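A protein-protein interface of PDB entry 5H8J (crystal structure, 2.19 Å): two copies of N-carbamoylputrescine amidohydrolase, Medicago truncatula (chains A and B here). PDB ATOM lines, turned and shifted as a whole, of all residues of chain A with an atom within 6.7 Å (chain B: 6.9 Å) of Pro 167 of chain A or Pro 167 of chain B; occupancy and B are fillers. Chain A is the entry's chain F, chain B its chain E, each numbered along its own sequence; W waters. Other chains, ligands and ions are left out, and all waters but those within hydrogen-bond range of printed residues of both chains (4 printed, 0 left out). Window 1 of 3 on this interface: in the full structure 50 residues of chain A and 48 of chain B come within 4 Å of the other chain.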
ATOM      1  N   ASP A 163     -27.526  16.316  13.031  1.00  0.00           N
ATOM      2  CA  ASP A 163     -27.058  15.271  13.957  1.00  0.00           C
ATOM      3  C   ASP A 163     -27.716  13.929  13.623  1.00  0.00           C
ATOM      4  O   ASP A 163     -27.151  12.893  13.862  1.00  0.00           O
ATOM      5  CB  ASP A 163     -27.419  15.593  15.428  1.00  0.00           C
ATOM      6  CG  ASP A 163     -26.635  16.732  16.006  1.00  0.00           C
ATOM      7  OD1 ASP A 163     -25.459  16.929  15.589  1.00  0.00           O
ATOM      8  OD2 ASP A 163     -27.175  17.440  16.899  1.00  0.00           O
ATOM      9  N   GLN A 164     -28.915  13.966  13.071  1.00  0.00           N
ATOM     10  CA  GLN A 164     -29.652  12.737  12.755  1.00  0.00           C
ATOM     11  C   GLN A 164     -28.994  11.828  11.682  1.00  0.00           C
ATOM     12  O   GLN A 164     -29.397  10.656  11.530  1.00  0.00           O
ATOM     13  CB  GLN A 164     -31.086  13.078  12.350  1.00  0.00           C
ATOM     14  CG  GLN A 164     -31.252  13.573  10.917  1.00  0.00           C
ATOM     15  CD  GLN A 164     -32.454  14.520  10.724  1.00  0.00           C
ATOM     16  OE1 GLN A 164     -32.411  15.467   9.877  1.00  0.00           O
ATOM     17  NE2 GLN A 164     -33.522  14.295  11.505  1.00  0.00           N
ATOM     18  N   TRP A 165     -28.005  12.339  10.961  1.00  0.00           N
ATOM     19  CA  TRP A 165     -27.334  11.561   9.924  1.00  0.00           C
ATOM     20  C   TRP A 165     -26.110  10.768  10.441  1.00  0.00           C
ATOM     21  O   TRP A 165     -25.460   9.997   9.670  1.00  0.00           O
ATOM     22  CB  TRP A 165     -26.880  12.502   8.810  1.00  0.00           C
ATOM     23  CG  TRP A 165     -28.028  13.114   8.021  1.00  0.00           C
ATOM     24  CD1 TRP A 165     -28.735  14.246   8.328  1.00  0.00           C
ATOM     25  CD2 TRP A 165     -28.582  12.614   6.793  1.00  0.00           C
ATOM     26  NE1 TRP A 165     -29.707  14.477   7.365  1.00  0.00           N
ATOM     27  CE2 TRP A 165     -29.632  13.489   6.417  1.00  0.00           C
ATOM     28  CE3 TRP A 165     -28.300  11.502   5.983  1.00  0.00           C
ATOM     29  CZ2 TRP A 165     -30.383  13.299   5.268  1.00  0.00           C
ATOM     30  CZ3 TRP A 165     -29.044  11.304   4.856  1.00  0.00           C
ATOM     31  CH2 TRP A 165     -30.081  12.210   4.495  1.00  0.00           C
ATOM     32  N   PHE A 166     -25.804  10.937  11.728  1.00  0.00           N
ATOM     33  CA  PHE A 166     -24.612  10.345  12.354  1.00  0.00           C
ATOM     34  C   PHE A 166     -24.938   9.224  13.372  1.00  0.00           C
ATOM     35  O   PHE A 166     -25.480   9.484  14.483  1.00  0.00           O
ATOM     36  CB  PHE A 166     -23.761  11.446  13.028  1.00  0.00           C
ATOM     37  CG  PHE A 166     -23.299  12.527  12.073  1.00  0.00           C
ATOM     38  CD1 PHE A 166     -24.137  13.563  11.722  1.00  0.00           C
ATOM     39  CD2 PHE A 166     -22.017  12.486  11.515  1.00  0.00           C
ATOM     40  CE1 PHE A 166     -23.711  14.563  10.824  1.00  0.00           C
ATOM     41  CE2 PHE A 166     -21.590  13.468  10.630  1.00  0.00           C
ATOM     42  CZ  PHE A 166     -22.439  14.507  10.282  1.00  0.00           C
ATOM     43  N   PRO A 167     -24.596   7.977  13.021  1.00  0.00           N
ATOM     44  CA  PRO A 167     -24.811   6.848  13.962  1.00  0.00           C
ATOM     45  C   PRO A 167     -24.186   7.084  15.312  1.00  0.00           C
ATOM     46  O   PRO A 167     -24.717   6.625  16.323  1.00  0.00           O
ATOM     47  CB  PRO A 167     -24.107   5.706  13.269  1.00  0.00           C
ATOM     48  CG  PRO A 167     -24.274   6.046  11.775  1.00  0.00           C
ATOM     49  CD  PRO A 167     -24.026   7.518  11.747  1.00  0.00           C
ATOM     50  N   GLU A 168     -23.070   7.796  15.323  1.00  0.00           N
ATOM     51  CA  GLU A 168     -22.330   8.066  16.516  1.00  0.00           C
ATOM     52  C   GLU A 168     -23.182   8.731  17.557  1.00  0.00           C
ATOM     53  O   GLU A 168     -23.085   8.402  18.768  1.00  0.00           O
ATOM     54  CB  GLU A 168     -21.122   8.974  16.236  1.00  0.00           C
ATOM     55  CG  GLU A 168     -19.973   8.331  15.462  1.00  0.00           C
ATOM     56  CD  GLU A 168     -19.994   8.533  13.952  1.00  0.00           C
ATOM     57  OE1 GLU A 168     -21.082   8.774  13.399  1.00  0.00           O
ATOM     58  OE2 GLU A 168     -18.912   8.429  13.322  1.00  0.00           O
ATOM     59  N   ALA A 169     -24.027   9.665  17.106  1.00  0.00           N
ATOM     60  CA  ALA A 169     -24.843  10.443  18.048  1.00  0.00           C
ATOM     61  C   ALA A 169     -25.872   9.570  18.662  1.00  0.00           C
ATOM     62  O   ALA A 169     -26.108   9.655  19.873  1.00  0.00           O
ATOM     63  CB  ALA A 169     -25.533  11.613  17.348  1.00  0.00           C
ATOM     64  N   ALA A 170     -26.501   8.727  17.836  1.00  0.00           N
ATOM     65  CA  ALA A 170     -27.548   7.841  18.357  1.00  0.00           C
ATOM     66  C   ALA A 170     -26.987   6.867  19.364  1.00  0.00           C
ATOM     67  O   ALA A 170     -27.547   6.669  20.373  1.00  0.00           O
ATOM     68  CB  ALA A 170     -28.228   7.100  17.248  1.00  0.00           C
ATOM     69  N   ARG A 171     -25.859   6.268  19.045  1.00  0.00           N
ATOM     70  CA  ARG A 171     -25.193   5.318  19.907  1.00  0.00           C
ATOM     71  C   ARG A 171     -24.746   5.939  21.242  1.00  0.00           C
ATOM     72  O   ARG A 171     -24.863   5.290  22.301  1.00  0.00           O
ATOM     73  CB  ARG A 171     -23.976   4.707  19.199  1.00  0.00           C
ATOM     74  CG  ARG A 171     -23.273   3.618  20.047  1.00  0.00           C
ATOM     75  CD  ARG A 171     -24.141   2.376  20.122  1.00  0.00           C
ATOM     76  NE  ARG A 171     -23.696   1.371  19.199  1.00  0.00           N
ATOM     77  CZ  ARG A 171     -24.447   0.365  18.767  1.00  0.00           C
ATOM     78  NH1 ARG A 171     -25.714   0.266  19.146  1.00  0.00           N
ATOM     79  NH2 ARG A 171     -23.940  -0.525  17.937  1.00  0.00           N
ATOM     80  N   ALA A 172     -24.227   7.167  21.180  1.00  0.00           N
ATOM     81  CA  ALA A 172     -23.773   7.890  22.364  1.00  0.00           C
ATOM     82  C   ALA A 172     -24.897   8.130  23.291  1.00  0.00           C
ATOM     83  O   ALA A 172     -24.720   8.025  24.505  1.00  0.00           O
ATOM     84  CB  ALA A 172     -23.151   9.218  21.973  1.00  0.00           C
ATOM     85  N   TYR A 183     -35.476  13.911  17.183  1.00  0.00           N
ATOM     86  CA  TYR A 183     -34.744  14.764  16.256  1.00  0.00           C
ATOM     87  C   TYR A 183     -35.606  15.861  15.549  1.00  0.00           C
ATOM     88  O   TYR A 183     -36.214  15.590  14.553  1.00  0.00           O
ATOM     89  CB  TYR A 183     -34.100  13.925  15.195  1.00  0.00           C
ATOM     90  CG  TYR A 183     -33.055  12.947  15.639  1.00  0.00           C
ATOM     91  CD1 TYR A 183     -33.398  11.653  16.006  1.00  0.00           C
ATOM     92  CD2 TYR A 183     -31.732  13.290  15.660  1.00  0.00           C
ATOM     93  CE1 TYR A 183     -32.447  10.738  16.403  1.00  0.00           C
ATOM     94  CE2 TYR A 183     -30.754  12.379  16.056  1.00  0.00           C
ATOM     95  CZ  TYR A 183     -31.132  11.097  16.419  1.00  0.00           C
ATOM     96  OH  TYR A 183     -30.187  10.207  16.788  1.00  0.00           O
ATOM     97  N   VAL A 205     -31.589   6.315   6.989  1.00  0.00           N
ATOM     98  CA  VAL A 205     -30.487   6.529   7.939  1.00  0.00           C
ATOM     99  C   VAL A 205     -30.981   6.510   9.413  1.00  0.00           C
ATOM    100  O   VAL A 205     -30.326   5.874  10.283  1.00  0.00           O
ATOM    101  CB  VAL A 205     -29.689   7.794   7.628  1.00  0.00           C
ATOM    102  CG1 VAL A 205     -28.796   8.168   8.787  1.00  0.00           C
ATOM    103  CG2 VAL A 205     -28.862   7.578   6.362  1.00  0.00           C
ATOM    104  N   GLY A 208     -32.178   3.202  10.542  1.00  0.00           N
ATOM    105  CA  GLY A 208     -30.982   2.474  10.897  1.00  0.00           C
ATOM    106  C   GLY A 208     -30.600   2.670  12.368  1.00  0.00           C
ATOM    107  O   GLY A 208     -30.275   1.702  13.056  1.00  0.00           O
ATOM    108  N   HIS A 209     -30.619   3.924  12.835  1.00  0.00           N
ATOM    109  CA  HIS A 209     -30.281   4.218  14.221  1.00  0.00           C
ATOM    110  C   HIS A 209     -31.240   3.501  15.182  1.00  0.00           C
ATOM    111  O   HIS A 209     -30.805   2.932  16.162  1.00  0.00           O
ATOM    112  CB  HIS A 209     -30.368   5.682  14.572  1.00  0.00           C
ATOM    113  CG  HIS A 209     -29.584   6.608  13.672  1.00  0.00           C
ATOM    114  ND1 HIS A 209     -28.445   6.227  12.997  1.00  0.00           N
ATOM    115  CD2 HIS A 209     -29.771   7.912  13.390  1.00  0.00           C
ATOM    116  CE1 HIS A 209     -27.978   7.253  12.313  1.00  0.00           C
ATOM    117  NE2 HIS A 209     -28.767   8.293  12.531  1.00  0.00           N
ATOM    118  N   ALA A 212     -30.487  -0.215  15.094  1.00  0.00           N
ATOM    119  CA  ALA A 212     -29.197  -0.595  15.626  1.00  0.00           C
ATOM    120  C   ALA A 212     -29.077  -0.472  17.138  1.00  0.00           C
ATOM    121  O   ALA A 212     -28.250  -1.190  17.735  1.00  0.00           O
ATOM    122  CB  ALA A 212     -28.065   0.152  14.981  1.00  0.00           C
ATOM    123  N   ASN A 213     -29.855   0.432  17.738  1.00  0.00           N
ATOM    124  CA  ASN A 213     -29.812   0.675  19.181  1.00  0.00           C
ATOM    125  C   ASN A 213     -31.023   0.062  19.946  1.00  0.00           C
ATOM    126  O   ASN A 213     -31.021   0.036  21.173  1.00  0.00           O
ATOM    127  CB  ASN A 213     -29.723   2.177  19.438  1.00  0.00           C
ATOM    128  CG  ASN A 213     -28.396   2.749  18.993  1.00  0.00           C
ATOM    129  OD1 ASN A 213     -27.404   2.620  19.683  1.00  0.00           O
ATOM    130  ND2 ASN A 213     -28.370   3.374  17.811  1.00  0.00           N
ATOM    131  N   LEU A 294     -12.661   5.507  15.331  1.00  0.00           N
ATOM    132  CA  LEU A 294     -13.792   6.448  15.300  1.00  0.00           C
ATOM    133  C   LEU A 294     -13.394   7.821  15.901  1.00  0.00           C
ATOM    134  O   LEU A 294     -14.132   8.791  15.773  1.00  0.00           O
ATOM    135  CB  LEU A 294     -15.034   5.918  15.988  1.00  0.00           C
ATOM    136  CG  LEU A 294     -15.561   4.532  15.581  1.00  0.00           C
ATOM    137  CD1 LEU A 294     -16.837   4.179  16.351  1.00  0.00           C
ATOM    138  CD2 LEU A 294     -15.776   4.432  14.079  1.00  0.00           C
ATOM    139  N   ASP B 163     -21.308  -8.826  12.696  1.00  0.00           N
ATOM    140  CA  ASP B 163     -20.691  -7.469  12.563  1.00  0.00           C
ATOM    141  C   ASP B 163     -21.645  -6.485  11.851  1.00  0.00           C
ATOM    142  O   ASP B 163     -21.573  -5.310  12.097  1.00  0.00           O
ATOM    143  CB  ASP B 163     -19.409  -7.462  11.714  1.00  0.00           C
ATOM    144  CG  ASP B 163     -18.210  -8.125  12.378  1.00  0.00           C
ATOM    145  OD1 ASP B 163     -18.138  -8.147  13.652  1.00  0.00           O
ATOM    146  OD2 ASP B 163     -17.323  -8.628  11.609  1.00  0.00           O
ATOM    147  N   GLN B 164     -22.522  -6.993  10.974  1.00  0.00           N
ATOM    148  CA  GLN B 164     -23.446  -6.155  10.182  1.00  0.00           C
ATOM    149  C   GLN B 164     -24.435  -5.348  10.998  1.00  0.00           C
ATOM    150  O   GLN B 164     -25.046  -4.450  10.492  1.00  0.00           O
ATOM    151  CB  GLN B 164     -24.189  -6.997   9.100  1.00  0.00           C
ATOM    152  CG  GLN B 164     -25.292  -7.871   9.637  1.00  0.00           C
ATOM    153  CD  GLN B 164     -25.543  -9.163   8.857  1.00  0.00           C
ATOM    154  OE1 GLN B 164     -26.009 -10.112   9.417  1.00  0.00           O
ATOM    155  NE2 GLN B 164     -25.236  -9.179   7.557  1.00  0.00           N
ATOM    156  N   TRP B 165     -24.594  -5.658  12.255  1.00  0.00           N
ATOM    157  CA  TRP B 165     -25.550  -4.927  13.089  1.00  0.00           C
ATOM    158  C   TRP B 165     -24.935  -3.682  13.749  1.00  0.00           C
ATOM    159  O   TRP B 165     -25.667  -2.841  14.339  1.00  0.00           O
ATOM    160  CB  TRP B 165     -26.099  -5.863  14.163  1.00  0.00           C
ATOM    161  CG  TRP B 165     -26.992  -6.977  13.611  1.00  0.00           C
ATOM    162  CD1 TRP B 165     -26.594  -8.211  13.142  1.00  0.00           C
ATOM    163  CD2 TRP B 165     -28.430  -6.962  13.480  1.00  0.00           C
ATOM    164  NE1 TRP B 165     -27.709  -8.961  12.723  1.00  0.00           N
ATOM    165  CE2 TRP B 165     -28.831  -8.214  12.919  1.00  0.00           C
ATOM    166  CE3 TRP B 165     -29.407  -6.025  13.768  1.00  0.00           C
ATOM    167  CZ2 TRP B 165     -30.160  -8.517  12.654  1.00  0.00           C
ATOM    168  CZ3 TRP B 165     -30.714  -6.339  13.506  1.00  0.00           C
ATOM    169  CH2 TRP B 165     -31.085  -7.582  12.961  1.00  0.00           C
ATOM    170  N   PHE B 166     -23.598  -3.556  13.651  1.00  0.00           N
ATOM    171  CA  PHE B 166     -22.850  -2.518  14.336  1.00  0.00           C
ATOM    172  C   PHE B 166     -22.426  -1.340  13.385  1.00  0.00           C
ATOM    173  O   PHE B 166     -21.603  -1.530  12.470  1.00  0.00           O
ATOM    174  CB  PHE B 166     -21.637  -3.176  15.021  1.00  0.00           C
ATOM    175  CG  PHE B 166     -22.055  -4.182  16.083  1.00  0.00           C
ATOM    176  CD1 PHE B 166     -22.400  -5.502  15.722  1.00  0.00           C
ATOM    177  CD2 PHE B 166     -22.156  -3.810  17.388  1.00  0.00           C
ATOM    178  CE1 PHE B 166     -22.833  -6.449  16.710  1.00  0.00           C
ATOM    179  CE2 PHE B 166     -22.583  -4.726  18.372  1.00  0.00           C
ATOM    180  CZ  PHE B 166     -22.916  -6.030  18.026  1.00  0.00           C
ATOM    181  N   PRO B 167     -23.007  -0.145  13.604  1.00  0.00           N
ATOM    182  CA  PRO B 167     -22.623   1.045  12.832  1.00  0.00           C
ATOM    183  C   PRO B 167     -21.156   1.345  13.003  1.00  0.00           C
ATOM    184  O   PRO B 167     -20.562   1.886  12.122  1.00  0.00           O
ATOM    185  CB  PRO B 167     -23.489   2.149  13.437  1.00  0.00           C
ATOM    186  CG  PRO B 167     -24.698   1.402  13.923  1.00  0.00           C
ATOM    187  CD  PRO B 167     -24.134   0.158  14.519  1.00  0.00           C
ATOM    188  N   GLU B 168     -20.585   0.987  14.139  1.00  0.00           N
ATOM    189  CA  GLU B 168     -19.172   1.242  14.369  1.00  0.00           C
ATOM    190  C   GLU B 168     -18.298   0.509  13.353  1.00  0.00           C
ATOM    191  O   GLU B 168     -17.288   1.083  12.891  1.00  0.00           O
ATOM    192  CB  GLU B 168     -18.711   0.854  15.782  1.00  0.00           C
ATOM    193  CG  GLU B 168     -19.313   1.628  16.946  1.00  0.00           C
ATOM    194  CD  GLU B 168     -20.595   1.034  17.489  1.00  0.00           C
ATOM    195  OE1 GLU B 168     -21.277   0.269  16.746  1.00  0.00           O
ATOM    196  OE2 GLU B 168     -20.914   1.316  18.675  1.00  0.00           O
ATOM    197  N   ALA B 169     -18.665  -0.740  12.998  1.00  0.00           N
ATOM    198  CA  ALA B 169     -17.863  -1.504  12.063  1.00  0.00           C
ATOM    199  C   ALA B 169     -17.911  -0.873  10.661  1.00  0.00           C
ATOM    200  O   ALA B 169     -16.870  -0.732  10.005  1.00  0.00           O
ATOM    201  CB  ALA B 169     -18.328  -2.956  11.988  1.00  0.00           C
ATOM    202  N   ALA B 170     -19.105  -0.509  10.210  1.00  0.00           N
ATOM    203  CA  ALA B 170     -19.238   0.091   8.853  1.00  0.00           C
ATOM    204  C   ALA B 170     -18.534   1.438   8.796  1.00  0.00           C
ATOM    205  O   ALA B 170     -17.906   1.796   7.744  1.00  0.00           O
ATOM    206  CB  ALA B 170     -20.695   0.235   8.440  1.00  0.00           C
ATOM    207  N   ARG B 171     -18.614   2.182   9.900  1.00  0.00           N
ATOM    208  CA  ARG B 171     -17.999   3.479   9.951  1.00  0.00           C
ATOM    209  C   ARG B 171     -16.460   3.322   9.943  1.00  0.00           C
ATOM    210  O   ARG B 171     -15.741   4.088   9.252  1.00  0.00           O
ATOM    211  CB  ARG B 171     -18.452   4.270  11.172  1.00  0.00           C
ATOM    212  CG  ARG B 171     -17.803   5.632  11.240  1.00  0.00           C
ATOM    213  CD  ARG B 171     -18.338   6.578  10.119  1.00  0.00           C
ATOM    214  NE  ARG B 171     -19.312   7.556  10.643  1.00  0.00           N
ATOM    215  CZ  ARG B 171     -20.269   8.139   9.916  1.00  0.00           C
ATOM    216  NH1 ARG B 171     -20.416   7.830   8.628  1.00  0.00           N
ATOM    217  NH2 ARG B 171     -21.084   9.021  10.477  1.00  0.00           N
ATOM    218  N   ALA B 172     -15.962   2.362  10.709  1.00  0.00           N
ATOM    219  CA  ALA B 172     -14.519   2.119  10.781  1.00  0.00           C
ATOM    220  C   ALA B 172     -13.944   1.811   9.362  1.00  0.00           C
ATOM    221  O   ALA B 172     -12.881   2.347   8.967  1.00  0.00           O
ATOM    222  CB  ALA B 172     -14.205   0.975  11.758  1.00  0.00           C
ATOM    223  N   TYR B 183     -20.868  -8.179   3.593  1.00  0.00           N
ATOM    224  CA  TYR B 183     -21.185  -8.977   4.792  1.00  0.00           C
ATOM    225  C   TYR B 183     -21.762 -10.347   4.443  1.00  0.00           C
ATOM    226  O   TYR B 183     -22.966 -10.473   4.132  1.00  0.00           O
ATOM    227  CB  TYR B 183     -22.207  -8.253   5.703  1.00  0.00           C
ATOM    228  CG  TYR B 183     -21.788  -6.882   6.231  1.00  0.00           C
ATOM    229  CD1 TYR B 183     -22.054  -5.721   5.509  1.00  0.00           C
ATOM    230  CD2 TYR B 183     -21.145  -6.759   7.436  1.00  0.00           C
ATOM    231  CE1 TYR B 183     -21.690  -4.476   5.993  1.00  0.00           C
ATOM    232  CE2 TYR B 183     -20.785  -5.534   7.926  1.00  0.00           C
ATOM    233  CZ  TYR B 183     -21.067  -4.391   7.182  1.00  0.00           C
ATOM    234  OH  TYR B 183     -20.712  -3.192   7.686  1.00  0.00           O
ATOM    235  N   VAL B 205     -31.146  -2.090   9.360  1.00  0.00           N
ATOM    236  CA  VAL B 205     -29.943  -1.696  10.038  1.00  0.00           C
ATOM    237  C   VAL B 205     -28.787  -1.548   9.015  1.00  0.00           C
ATOM    238  O   VAL B 205     -28.006  -0.598   9.070  1.00  0.00           O
ATOM    239  CB  VAL B 205     -29.606  -2.696  11.131  1.00  0.00           C
ATOM    240  CG1 VAL B 205     -28.199  -2.468  11.682  1.00  0.00           C
ATOM    241  CG2 VAL B 205     -30.642  -2.605  12.250  1.00  0.00           C
ATOM    242  N   GLY B 208     -29.080   1.375   6.790  1.00  0.00           N
ATOM    243  CA  GLY B 208     -28.654   2.527   7.542  1.00  0.00           C
ATOM    244  C   GLY B 208     -27.151   2.768   7.404  1.00  0.00           C
ATOM    245  O   GLY B 208     -26.718   3.916   7.232  1.00  0.00           O
ATOM    246  N   HIS B 209     -26.358   1.690   7.488  1.00  0.00           N
ATOM    247  CA  HIS B 209     -24.937   1.828   7.331  1.00  0.00           C
ATOM    248  C   HIS B 209     -24.585   2.336   5.939  1.00  0.00           C
ATOM    249  O   HIS B 209     -23.687   3.210   5.792  1.00  0.00           O
ATOM    250  CB  HIS B 209     -24.179   0.536   7.489  1.00  0.00           C
ATOM    251  CG  HIS B 209     -24.477  -0.210   8.735  1.00  0.00           C
ATOM    252  ND1 HIS B 209     -24.812   0.406   9.922  1.00  0.00           N
ATOM    253  CD2 HIS B 209     -24.456  -1.527   8.983  1.00  0.00           C
ATOM    254  CE1 HIS B 209     -25.018  -0.509  10.841  1.00  0.00           C
ATOM    255  NE2 HIS B 209     -24.794  -1.690  10.300  1.00  0.00           N
ATOM    256  N   ALA B 212     -25.625   6.115   5.766  1.00  0.00           N
ATOM    257  CA  ALA B 212     -24.852   6.985   6.644  1.00  0.00           C
ATOM    258  C   ALA B 212     -23.411   7.166   6.196  1.00  0.00           C
ATOM    259  O   ALA B 212     -22.778   8.176   6.540  1.00  0.00           O
ATOM    260  CB  ALA B 212     -24.871   6.433   8.078  1.00  0.00           C
ATOM    261  N   ASN B 213     -22.878   6.207   5.462  1.00  0.00           N
ATOM    262  CA  ASN B 213     -21.502   6.286   4.986  1.00  0.00           C
ATOM    263  C   ASN B 213     -21.421   6.560   3.509  1.00  0.00           C
ATOM    264  O   ASN B 213     -20.330   6.783   2.989  1.00  0.00           O
ATOM    265  CB  ASN B 213     -20.725   5.024   5.343  1.00  0.00           C
ATOM    266  CG  ASN B 213     -20.620   4.814   6.874  1.00  0.00           C
ATOM    267  OD1 ASN B 213     -19.817   5.437   7.547  1.00  0.00           O
ATOM    268  ND2 ASN B 213     -21.425   3.937   7.390  1.00  0.00           N
ATOM    269  N   LEU B 294     -18.153   6.287  23.005  1.00  0.00           N
ATOM    270  CA  LEU B 294     -18.241   5.073  22.228  1.00  0.00           C
ATOM    271  C   LEU B 294     -17.135   4.090  22.594  1.00  0.00           C
ATOM    272  O   LEU B 294     -17.202   2.941  22.206  1.00  0.00           O
ATOM    273  CB  LEU B 294     -18.172   5.343  20.707  1.00  0.00           C
ATOM    274  CG  LEU B 294     -19.126   6.376  20.100  1.00  0.00           C
ATOM    275  CD1 LEU B 294     -18.945   6.438  18.601  1.00  0.00           C
ATOM    276  CD2 LEU B 294     -20.542   5.982  20.409  1.00  0.00           C
HETATM  277  O   HOH W   1     -27.946   1.314  11.392  1.00  0.00           O
HETATM  278  O   HOH W   2     -23.012   9.886   8.612  1.00  0.00           O
HETATM  279  O   HOH W   3     -25.914  -2.442  17.123  1.00  0.00           O
HETATM  280  O   HOH W   4     -27.724   4.594   9.984  1.00  0.00           O
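Phe 166 of chain A touches Arg 171 of chain B. Pro 167 of chain A touches Pro 167 of chain B (CB to CB, 3.6 Å). NH2 of Arg 171 of chain B touches CD of Pro 167 of chain A, 3.5 Å away. Arg 171 of chain A touches Phe 166 of chain B (NH2 to CD2, 3.8 Å). Pro 167 of chain B touches Arg 171 of chain A. Leu 294 of chain B touches Ala 172 of chain A. Ala 212 of chain B touches Val 205 of chain A. O of Trp 165 of chain B touches CB of Ala 212 of chain A (3.9 Å). Glu 168 of chain B touches Leu 294 of chain A (CG to CD1, 3.6 Å). Leu 294 of chain A touches Leu 294 of chain B.
Water W2 lies within hydrogen-bond range of O of Trp 165 of chain A (2.7 Å), O of Ala 212 of chain B (2.7 Å) and NH2 of Arg 171 of chain B (2.8 Å). Water W3 lies within hydrogen-bond range of O of Ala 212 of chain A (2.7 Å), O of Trp 165 of chain B (2.8 Å) and NH2 of Arg 171 of chain A (2.9 Å). Water W1 bridges the backbone carbonyl oxygen of Gly 208 of chain A (2.9 Å) and the backbone carbonyl oxygen of Val 205 of chain B (3.0 Å). Water W4 bridges the backbone carbonyl oxygen (O) of Val 205 of chain A and the backbone carbonyl oxygen (O) of Gly 208 of chain B.
The side-chain carboxylate (OE2) of Glu 168 of chain B lies within salt-bridge range of the guanidinium group (NE) of Arg 171 of chain A, at 2.8 Å. The guanidinium group of Arg 171 of chain B is in salt-bridge range of the side-chain carboxylate of Glu 168 of chain A (2.8 Å).
The backbone carbonyl oxygen (O) of Ala 212 of chain B lies within hydrogen-bond range of the guanidinium group (NH1) of Arg 171 of chain B (3.2 Å). The guanidinium group (NH1) of Arg 171 of chain B sits at hydrogen-bond distance from the side-chain amide oxygen (OD1) of Asn 213 of chain B (2.7 Å). O of Val 205 of chain B is in hydrogen-bond range of ND1 of His 209 of chain B (3.5 Å). The backbone carbonyl oxygen (O) of Ala 212 of chain A sits at hydrogen-bond distance from the guanidinium group (NH1) of Arg 171 of chain A. The guanidinium group (NH1) of Arg 171 of chain A sits at hydrogen-bond distance from the side-chain amide oxygen (OD1) of Asn 213 of chain A (2.9 Å). The backbone carbonyl oxygen of Val 205 of chain A lies within hydrogen-bond range of a ring nitrogen (ND1) of His 209 of chain A (3.3 Å).
Of the printed residues of chain B, Trp 165 of chain A touches Ala 212. Printed residues of chain B within 4 Å of Phe 166 of chain A: Arg 171 (3.7 Å). Pro 167 of chain A touches just these residues of chain B: Pro 167 (3.6 Å), Arg 171 (3.5 Å) and Ala 212 (3.8 Å). Of the printed residues of chain B, Glu 168 of chain A touches Arg 171 and Leu 294. Pro 167 of chain B touches just these residues of chain A: Pro 167, Arg 171 and Ala 212. Of the printed residues of chain A, Ala 212 of chain B touches Trp 165, Pro 167 and Val 205. The nearest residue of chain B that does not touch Pro 167 of chain A is Gly 208 of chain B (5.6 Å). The nearest printed residue of chain B that does not touch Val 205 of chain A is Gly 208 of chain B (4.3 Å).
Pro 167 of chain B touches its own counterpart, Pro 167 of chain A. Glu 168 of chain A touches Leu 294 of chain B, and with the chains exchanged Leu 294 of chain A touches Glu 168 of chain B. Val 205 of chain A touches Ala 212 of chain B, and with the chains exchanged Ala 212 of chain A touches Val 205 of chain B. Leu 294 of chain A touches its own counterpart, Leu 294 of chain B. Positions printed for both chains: 163, 164, 165, 166, 167, 168, 169, 170, 171, 172, 183, 205, 208, 209, 212, 213 and 294.
Hydrophobic or aromatic side chains of chain A within 4 Å of the printed part of chain B: Phe 166, Pro 167, Val 205, Ala 212 and Leu 294. Printed residues of chain B that touch a printed residue of chain A: Trp 165, Phe 166, Pro 167, Glu 168, Arg 171, Ala 172, Val 205, Ala 212 and Leu 294. Among the printed residues, Asp or Glu carboxylates within 4 Å of a Lys or Arg side-chain nitrogen of the other chain: Glu 168 of chain A with Arg 171 of chain B (2.8 Å) and Arg 171 of chain A with Glu 168 of chain B (2.8 Å).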
